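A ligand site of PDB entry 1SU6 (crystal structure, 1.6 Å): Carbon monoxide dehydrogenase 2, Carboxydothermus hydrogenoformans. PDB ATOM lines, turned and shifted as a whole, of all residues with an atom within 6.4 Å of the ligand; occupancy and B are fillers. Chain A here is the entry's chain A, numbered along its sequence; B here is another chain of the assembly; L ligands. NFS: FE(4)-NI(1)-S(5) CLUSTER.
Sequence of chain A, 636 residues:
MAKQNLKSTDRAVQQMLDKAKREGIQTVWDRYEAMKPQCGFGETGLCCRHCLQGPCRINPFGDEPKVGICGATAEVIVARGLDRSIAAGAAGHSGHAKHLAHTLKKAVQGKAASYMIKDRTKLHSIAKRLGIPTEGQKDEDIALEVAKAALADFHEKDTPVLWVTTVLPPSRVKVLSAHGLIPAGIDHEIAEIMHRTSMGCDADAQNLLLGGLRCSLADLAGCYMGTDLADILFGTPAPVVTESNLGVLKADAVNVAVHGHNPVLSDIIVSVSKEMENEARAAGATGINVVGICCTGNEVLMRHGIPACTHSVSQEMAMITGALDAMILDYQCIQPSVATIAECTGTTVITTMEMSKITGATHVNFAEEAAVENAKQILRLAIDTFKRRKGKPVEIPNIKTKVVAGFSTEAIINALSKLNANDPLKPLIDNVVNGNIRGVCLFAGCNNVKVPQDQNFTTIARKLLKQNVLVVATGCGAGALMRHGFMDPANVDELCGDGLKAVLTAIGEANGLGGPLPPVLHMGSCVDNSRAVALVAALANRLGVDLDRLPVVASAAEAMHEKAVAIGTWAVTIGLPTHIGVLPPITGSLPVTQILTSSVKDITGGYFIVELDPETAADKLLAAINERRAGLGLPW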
ATOM      1  N   HIS A  93      23.029   7.834  21.416  1.00  0.00           N
ATOM      2  CA  HIS A  93      24.100   8.465  22.193  1.00  0.00           C
ATOM      3  C   HIS A  93      24.877   7.439  23.000  1.00  0.00           C
ATOM      4  O   HIS A  93      26.082   7.607  23.135  1.00  0.00           O
ATOM      5  CB  HIS A  93      23.529   9.542  23.127  1.00  0.00           C
ATOM      6  CG  HIS A  93      23.078  10.756  22.367  1.00  0.00           C
ATOM      7  ND1 HIS A  93      21.850  11.351  22.563  1.00  0.00           N
ATOM      8  CD2 HIS A  93      23.683  11.481  21.392  1.00  0.00           C
ATOM      9  CE1 HIS A  93      21.723  12.394  21.760  1.00  0.00           C
ATOM     10  NE2 HIS A  93      22.841  12.500  21.030  1.00  0.00           N
ATOM     11  N   GLY A 260      28.487  12.022  10.098  1.00  0.00           N
ATOM     12  CA  GLY A 260      28.112  11.047  11.135  1.00  0.00           C
ATOM     13  C   GLY A 260      28.449  11.661  12.492  1.00  0.00           C
ATOM     14  O   GLY A 260      28.232  12.859  12.712  1.00  0.00           O
ATOM     15  N   HIS A 261      28.972  10.843  13.406  1.00  0.00           N
ATOM     16  CA  HIS A 261      29.076  11.254  14.794  1.00  0.00           C
ATOM     17  C   HIS A 261      30.342  10.980  15.567  1.00  0.00           C
ATOM     18  O   HIS A 261      30.705  11.826  16.390  1.00  0.00           O
ATOM     19  CB  HIS A 261      27.933  10.493  15.592  1.00  0.00           C
ATOM     20  CG  HIS A 261      26.737  11.348  15.309  1.00  0.00           C
ATOM     21  ND1 HIS A 261      25.984  11.198  14.164  1.00  0.00           N
ATOM     22  CD2 HIS A 261      26.220  12.407  15.976  1.00  0.00           C
ATOM     23  CE1 HIS A 261      25.031  12.100  14.152  1.00  0.00           C
ATOM     24  NE2 HIS A 261      25.162  12.835  15.244  1.00  0.00           N
ATOM     25  N   CYS A 294      27.673  17.469   9.888  1.00  0.00           N
ATOM     26  CA  CYS A 294      26.913  17.009  11.061  1.00  0.00           C
ATOM     27  C   CYS A 294      27.805  16.878  12.278  1.00  0.00           C
ATOM     28  O   CYS A 294      28.770  17.668  12.415  1.00  0.00           O
ATOM     29  CB  CYS A 294      26.119  15.743  10.720  1.00  0.00           C
ATOM     30  SG  CYS A 294      24.360  16.103  10.341  1.00  0.00           S
ATOM     31  N   CYS A 295      27.575  15.986  13.249  1.00  0.00           N
ATOM     32  CA  CYS A 295      28.323  16.145  14.486  1.00  0.00           C
ATOM     33  C   CYS A 295      29.795  15.733  14.448  1.00  0.00           C
ATOM     34  O   CYS A 295      30.627  16.273  15.170  1.00  0.00           O
ATOM     35  CB  CYS A 295      27.689  15.331  15.631  1.00  0.00           C
ATOM     36  SG  CYS A 295      26.240  16.137  16.365  1.00  0.00           S
ATOM     37  N   THR A 296      30.159  14.728  13.647  1.00  0.00           N
ATOM     38  CA  THR A 296      31.581  14.356  13.639  1.00  0.00           C
ATOM     39  C   THR A 296      32.351  15.529  13.026  1.00  0.00           C
ATOM     40  O   THR A 296      33.508  15.753  13.375  1.00  0.00           O
ATOM     41  CB  THR A 296      31.802  13.032  12.901  1.00  0.00           C
ATOM     42  OG1 THR A 296      33.060  12.463  13.330  1.00  0.00           O
ATOM     43  CG2 THR A 296      31.916  13.225  11.404  1.00  0.00           C
ATOM     44  N   HIS A 311      25.350  21.019   7.251  1.00  0.00           N
ATOM     45  CA  HIS A 311      24.741  20.290   8.343  1.00  0.00           C
ATOM     46  C   HIS A 311      23.338  19.789   7.971  1.00  0.00           C
ATOM     47  O   HIS A 311      22.613  20.351   7.170  1.00  0.00           O
ATOM     48  CB  HIS A 311      24.558  21.145   9.619  1.00  0.00           C
ATOM     49  CG  HIS A 311      25.821  21.811  10.057  1.00  0.00           C
ATOM     50  ND1 HIS A 311      26.216  22.982   9.447  1.00  0.00           N
ATOM     51  CD2 HIS A 311      26.793  21.499  10.931  1.00  0.00           C
ATOM     52  CE1 HIS A 311      27.362  23.390   9.963  1.00  0.00           C
ATOM     53  NE2 HIS A 311      27.747  22.494  10.889  1.00  0.00           N
ATOM     54  N   SER A 312      22.962  18.721   8.642  1.00  0.00           N
ATOM     55  CA  SER A 312      21.593  18.258   8.766  1.00  0.00           C
ATOM     56  C   SER A 312      20.877  18.173   7.431  1.00  0.00           C
ATOM     57  O   SER A 312      21.285  17.473   6.499  1.00  0.00           O
ATOM     58  CB  SER A 312      20.884  19.242   9.719  1.00  0.00           C
ATOM     59  OG  SER A 312      19.688  18.657  10.196  1.00  0.00           O
ATOM     60  N   VAL A 313      19.787  18.928   7.347  1.00  0.00           N
ATOM     61  CA  VAL A 313      18.877  18.817   6.229  1.00  0.00           C
ATOM     62  C   VAL A 313      19.505  19.118   4.875  1.00  0.00           C
ATOM     63  O   VAL A 313      19.065  18.551   3.856  1.00  0.00           O
ATOM     64  CB  VAL A 313      17.664  19.755   6.458  1.00  0.00           C
ATOM     65  CG1 VAL A 313      17.998  21.226   6.291  1.00  0.00           C
ATOM     66  CG2 VAL A 313      16.525  19.387   5.517  1.00  0.00           C
ATOM     67  N   GLN A 332      24.385   7.661  12.183  1.00  0.00           N
ATOM     68  CA  GLN A 332      23.368   8.573  12.671  1.00  0.00           C
ATOM     69  C   GLN A 332      23.290   9.831  11.803  1.00  0.00           C
ATOM     70  O   GLN A 332      24.340  10.448  11.561  1.00  0.00           O
ATOM     71  CB  GLN A 332      23.585   9.004  14.113  1.00  0.00           C
ATOM     72  CG  GLN A 332      23.535   7.854  15.137  1.00  0.00           C
ATOM     73  CD  GLN A 332      24.148   8.246  16.481  1.00  0.00           C
ATOM     74  OE1 GLN A 332      24.231   9.425  16.841  1.00  0.00           O
ATOM     75  NE2 GLN A 332      24.598   7.243  17.247  1.00  0.00           N
ATOM     76  N   CYS A 333      22.070  10.147  11.385  1.00  0.00           N
ATOM     77  CA  CYS A 333      21.698  11.384  10.737  1.00  0.00           C
ATOM     78  C   CYS A 333      22.218  11.506   9.311  1.00  0.00           C
ATOM     79  O   CYS A 333      22.150  12.622   8.783  1.00  0.00           O
ATOM     80  CB  CYS A 333      22.196  12.603  11.566  1.00  0.00           C
ATOM     81  SG  CYS A 333      21.436  12.545  13.225  1.00  0.00           S
ATOM     82  N   ALA A 444      20.109  23.770  20.538  1.00  0.00           N
ATOM     83  CA  ALA A 444      20.592  22.423  20.273  1.00  0.00           C
ATOM     84  C   ALA A 444      19.758  21.773  19.176  1.00  0.00           C
ATOM     85  O   ALA A 444      18.735  22.319  18.782  1.00  0.00           O
ATOM     86  CB  ALA A 444      20.548  21.580  21.551  1.00  0.00           C
ATOM     87  N   GLY A 445      20.225  20.610  18.727  1.00  0.00           N
ATOM     88  CA  GLY A 445      19.372  19.803  17.868  1.00  0.00           C
ATOM     89  C   GLY A 445      19.500  20.193  16.402  1.00  0.00           C
ATOM     90  O   GLY A 445      20.359  20.954  16.002  1.00  0.00           O
ATOM     91  N   CYS A 446      18.610  19.650  15.617  1.00  0.00           N
ATOM     92  CA  CYS A 446      18.658  19.530  14.176  1.00  0.00           C
ATOM     93  C   CYS A 446      18.103  20.701  13.405  1.00  0.00           C
ATOM     94  O   CYS A 446      17.545  21.651  13.954  1.00  0.00           O
ATOM     95  CB  CYS A 446      17.778  18.277  13.828  1.00  0.00           C
ATOM     96  SG  CYS A 446      17.814  16.958  15.073  1.00  0.00           S
ATOM     97  N   ASN A 447      18.214  20.627  12.074  1.00  0.00           N
ATOM     98  CA  ASN A 447      17.266  21.246  11.174  1.00  0.00           C
ATOM     99  C   ASN A 447      16.151  20.241  10.835  1.00  0.00           C
ATOM    100  O   ASN A 447      16.339  19.036  11.018  1.00  0.00           O
ATOM    101  CB  ASN A 447      17.868  21.703   9.846  1.00  0.00           C
ATOM    102  CG  ASN A 447      18.891  22.815   9.973  1.00  0.00           C
ATOM    103  OD1 ASN A 447      18.625  23.923  10.451  1.00  0.00           O
ATOM    104  ND2 ASN A 447      20.065  22.464   9.475  1.00  0.00           N
ATOM    105  N   THR A 474      25.124  23.935  20.301  1.00  0.00           N
ATOM    106  CA  THR A 474      25.752  22.662  19.966  1.00  0.00           C
ATOM    107  C   THR A 474      25.106  22.043  18.711  1.00  0.00           C
ATOM    108  O   THR A 474      24.043  22.467  18.224  1.00  0.00           O
ATOM    109  CB  THR A 474      25.621  21.646  21.117  1.00  0.00           C
ATOM    110  OG1 THR A 474      24.209  21.437  21.334  1.00  0.00           O
ATOM    111  CG2 THR A 474      26.143  22.187  22.430  1.00  0.00           C
ATOM    112  N   GLY A 475      25.765  21.010  18.196  1.00  0.00           N
ATOM    113  CA  GLY A 475      25.225  20.250  17.089  1.00  0.00           C
ATOM    114  C   GLY A 475      24.839  21.104  15.918  1.00  0.00           C
ATOM    115  O   GLY A 475      25.535  22.026  15.480  1.00  0.00           O
ATOM    116  N   CYS A 476      23.659  20.829  15.361  1.00  0.00           N
ATOM    117  CA  CYS A 476      23.305  21.535  14.129  1.00  0.00           C
ATOM    118  C   CYS A 476      22.639  22.865  14.439  1.00  0.00           C
ATOM    119  O   CYS A 476      22.364  23.658  13.544  1.00  0.00           O
ATOM    120  CB  CYS A 476      22.448  20.620  13.238  1.00  0.00           C
ATOM    121  SG  CYS A 476      23.398  19.167  12.680  1.00  0.00           S
ATOM    122  N   GLY A 477      22.407  23.126  15.728  1.00  0.00           N
ATOM    123  CA  GLY A 477      21.976  24.453  16.165  1.00  0.00           C
ATOM    124  C   GLY A 477      23.237  25.350  16.069  1.00  0.00           C
ATOM    125  O   GLY A 477      23.119  26.458  15.531  1.00  0.00           O
ATOM    126  N   SER A 525      29.553  19.188  19.752  1.00  0.00           N
ATOM    127  CA  SER A 525      28.600  18.294  19.098  1.00  0.00           C
ATOM    128  C   SER A 525      27.345  18.080  19.920  1.00  0.00           C
ATOM    129  O   SER A 525      27.206  18.627  21.011  1.00  0.00           O
ATOM    130  CB  SER A 525      29.275  16.940  18.878  1.00  0.00           C
ATOM    131  OG  SER A 525      29.671  16.463  20.171  1.00  0.00           O
ATOM    132  N   CYS A 526      26.364  17.265  19.483  1.00  0.00           N
ATOM    133  CA  CYS A 526      25.237  17.070  20.406  1.00  0.00           C
ATOM    134  C   CYS A 526      25.594  16.293  21.666  1.00  0.00           C
ATOM    135  O   CYS A 526      24.961  16.586  22.697  1.00  0.00           O
ATOM    136  CB  CYS A 526      24.079  16.336  19.714  1.00  0.00           C
ATOM    137  SG  CYS A 526      23.596  17.192  18.206  1.00  0.00           S
ATOM    138  N   VAL A 527      26.541  15.349  21.649  1.00  0.00           N
ATOM    139  CA  VAL A 527      26.904  14.803  22.963  1.00  0.00           C
ATOM    140  C   VAL A 527      27.458  15.885  23.886  1.00  0.00           C
ATOM    141  O   VAL A 527      27.279  15.822  25.086  1.00  0.00           O
ATOM    142  CB  VAL A 527      27.921  13.646  22.906  1.00  0.00           C
ATOM    143  CG1 VAL A 527      27.216  12.400  22.357  1.00  0.00           C
ATOM    144  CG2 VAL A 527      29.165  13.980  22.090  1.00  0.00           C
ATOM    145  N   MET A 560      14.538  17.306  14.937  1.00  0.00           N
ATOM    146  CA  MET A 560      14.216  16.234  13.987  1.00  0.00           C
ATOM    147  C   MET A 560      14.360  14.837  14.583  1.00  0.00           C
ATOM    148  O   MET A 560      13.442  14.027  14.640  1.00  0.00           O
ATOM    149  CB  MET A 560      15.128  16.376  12.741  1.00  0.00           C
ATOM    150  CG  MET A 560      14.853  15.334  11.670  1.00  0.00           C
ATOM    151  SD  MET A 560      15.905  13.868  11.731  1.00  0.00           S
ATOM    152  CE  MET A 560      17.532  14.610  11.584  1.00  0.00           C
ATOM    153  N   HIS A 561      15.546  14.506  15.050  1.00  0.00           N
ATOM    154  CA  HIS A 561      15.918  13.136  15.389  1.00  0.00           C
ATOM    155  C   HIS A 561      15.366  12.678  16.723  1.00  0.00           C
ATOM    156  O   HIS A 561      15.116  13.499  17.625  1.00  0.00           O
ATOM    157  CB  HIS A 561      17.452  13.006  15.400  1.00  0.00           C
ATOM    158  CG  HIS A 561      17.952  11.605  15.217  1.00  0.00           C
ATOM    159  ND1 HIS A 561      18.049  10.690  16.230  1.00  0.00           N
ATOM    160  CD2 HIS A 561      18.412  10.974  14.112  1.00  0.00           C
ATOM    161  CE1 HIS A 561      18.544   9.537  15.786  1.00  0.00           C
ATOM    162  NE2 HIS A 561      18.760   9.702  14.479  1.00  0.00           N
ATOM    163  N   GLU A 562      15.196  11.357  16.851  1.00  0.00           N
ATOM    164  CA  GLU A 562      14.845  10.806  18.178  1.00  0.00           C
ATOM    165  C   GLU A 562      15.818  11.312  19.236  1.00  0.00           C
ATOM    166  O   GLU A 562      15.464  11.580  20.396  1.00  0.00           O
ATOM    167  CB  GLU A 562      14.793   9.271  18.095  1.00  0.00           C
ATOM    168  CG  GLU A 562      13.530   8.869  17.300  1.00  0.00           C
ATOM    169  CD  GLU A 562      13.521   7.397  16.922  1.00  0.00           C
ATOM    170  OE1 GLU A 562      14.546   6.858  16.475  1.00  0.00           O
ATOM    171  OE2 GLU A 562      12.426   6.789  17.058  1.00  0.00           O
ATOM    172  N   LYS A 563      17.096  11.447  18.850  1.00  0.00           N
ATOM    173  CA  LYS A 563      18.103  11.949  19.785  1.00  0.00           C
ATOM    174  C   LYS A 563      17.742  13.339  20.300  1.00  0.00           C
ATOM    175  O   LYS A 563      17.951  13.687  21.468  1.00  0.00           O
ATOM    176  CB  LYS A 563      19.471  12.019  19.116  1.00  0.00           C
ATOM    177  CG  LYS A 563      20.175  10.667  18.960  1.00  0.00           C
ATOM    178  CD  LYS A 563      21.518  10.852  18.263  1.00  0.00           C
ATOM    179  CE  LYS A 563      21.318  11.090  16.769  1.00  0.00           C
ATOM    180  NZ  LYS A 563      22.636  11.364  16.095  1.00  0.00           N
ATOM    181  N   ALA A 564      17.210  14.192  19.428  1.00  0.00           N
ATOM    182  CA  ALA A 564      16.843  15.542  19.867  1.00  0.00           C
ATOM    183  C   ALA A 564      15.677  15.481  20.836  1.00  0.00           C
ATOM    184  O   ALA A 564      15.576  16.273  21.758  1.00  0.00           O
ATOM    185  CB  ALA A 564      16.483  16.437  18.684  1.00  0.00           C
ATOM    186  N   ILE A 567      17.278  14.555  24.151  1.00  0.00           N
ATOM    187  CA  ILE A 567      17.951  15.728  24.751  1.00  0.00           C
ATOM    188  C   ILE A 567      16.947  16.718  25.327  1.00  0.00           C
ATOM    189  O   ILE A 567      17.107  17.241  26.460  1.00  0.00           O
ATOM    190  CB  ILE A 567      18.838  16.426  23.690  1.00  0.00           C
ATOM    191  CG1 ILE A 567      20.115  15.644  23.379  1.00  0.00           C
ATOM    192  CG2 ILE A 567      19.154  17.862  24.110  1.00  0.00           C
ATOM    193  CD1 ILE A 567      20.760  16.098  22.080  1.00  0.00           C
ATOM    194  N   MET B 199      16.988   7.358  12.793  1.00  0.00           N
ATOM    195  CA  MET B 199      17.130   8.042  11.501  1.00  0.00           C
ATOM    196  C   MET B 199      18.584   8.169  11.097  1.00  0.00           C
ATOM    197  O   MET B 199      19.492   8.413  11.894  1.00  0.00           O
ATOM    198  CB  MET B 199      16.459   9.418  11.612  1.00  0.00           C
ATOM    199  CG  MET B 199      16.491  10.189  10.298  1.00  0.00           C
ATOM    200  SD  MET B 199      18.019  11.141  10.175  1.00  0.00           S
ATOM    201  CE  MET B 199      17.599  12.263   8.833  1.00  0.00           C
HETATM  202 NI1  NFS L   1      21.993  15.823  16.954  1.00  0.00          NI
HETATM  203 FE1  NFS L   1      24.387  14.735  15.860  1.00  0.00          FE
HETATM  204 FE2  NFS L   1      22.526  17.156  13.493  1.00  0.00          FE
HETATM  205 FE3  NFS L   1      20.107  16.473  14.811  1.00  0.00          FE
HETATM  206 FE4  NFS L   1      21.645  14.662  13.889  1.00  0.00          FE
HETATM  207  S1  NFS L   1      23.763  15.339  13.764  1.00  0.00           S
HETATM  208  S2  NFS L   1      23.171  14.003  17.599  1.00  0.00           S
HETATM  209  S3  NFS L   1      20.429  14.621  15.882  1.00  0.00           S
HETATM  210  S4  NFS L   1      20.556  16.290  12.576  1.00  0.00           S
HETATM  211  S5  NFS L   1      21.691  17.806  15.631  1.00  0.00           S
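The backbone carbonyl oxygen of Gly 445 sits close to a sulfur (S5) of the ligand, at 3.4 Å.
Met 560 touches the ligand (CE to S4, 3.6 Å).
His 561 touches the ligand (CB to S3, 3.4 Å).
Hydrophobic or aromatic side chains within 4 Å of the ligand: His 261, Met 560 and His 561.
Within 4 Å of the ligand: His 93, His 261, Cys 294, Cys 295, Ser 312, Cys 333, Gly 445, Cys 446, Cys 476, Cys 526, Met 560, His 561 and Lys 563.
The nearest printed residue that does not touch the ligand is Gly 475 (4.5 Å).
NE2 of His 261 sits close to NZ of Lys 563, at 3.0 Å.
The side-chain sulfur of Cys 333 sits close to the side-chain amino group of Lys 563 (3.3 Å).
O of Gly 445 sits close to N of Cys 476 (3.4 Å).
The side-chain sulfur (SG) of Cys 446 sits close to the backbone NH (N) of Met 560 (3.3 Å).
The side-chain amino group (NZ) of Lys 563 is in hydrogen-bond range of the side-chain amide oxygen (OE1) of Gln 332 (2.6 Å).
The backbone NH of Gly 477 lies within hydrogen-bond range of the backbone carbonyl oxygen of Gly 445, at 3.0 Å.
The backbone NH (N) of Ser 312 sits at hydrogen-bond distance from the side-chain sulfur (SG) of Cys 294, at 3.4 Å.
The side-chain hydroxyl of Ser 312 is in hydrogen-bond range of the backbone NH of Asn 447.
FE1 of the ligand is bound by NE2 of His 261.
SG of Cys 333 is bound to FE4 of the ligand, 2.2 Å away.
The backbone NH (N) of Cys 476 sits close to a sulfur (S5) of the ligand, at 3.6 Å.
FE2 of the ligand is bound by SG of Cys 476, 2.3 Å away.
N of Cys 446 sits close to S5 of the ligand (3.6 Å).
FE3 of the ligand is bound by SG of Cys 446 (2.4 Å).
SG of Cys 295 is bound to FE1 of the ligand, at 2.4 Å.
The side-chain sulfur (SG) of Cys 526 is bound to a nickel atom (NI1) of the ligand (2.5 Å).
S2 of the ligand sits close to NZ of Lys 563, 3.1 Å away.
A sulfur (S4) of the ligand lies close to the side-chain hydroxyl (OG) of Ser 312.
The side-chain sulfur (SG) of Cys 294 lies close to a sulfur (S1) of the ligand (3.6 Å).
A ring nitrogen (NE2) of His 93 sits close to a sulfur (S2) of the ligand (3.8 Å).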
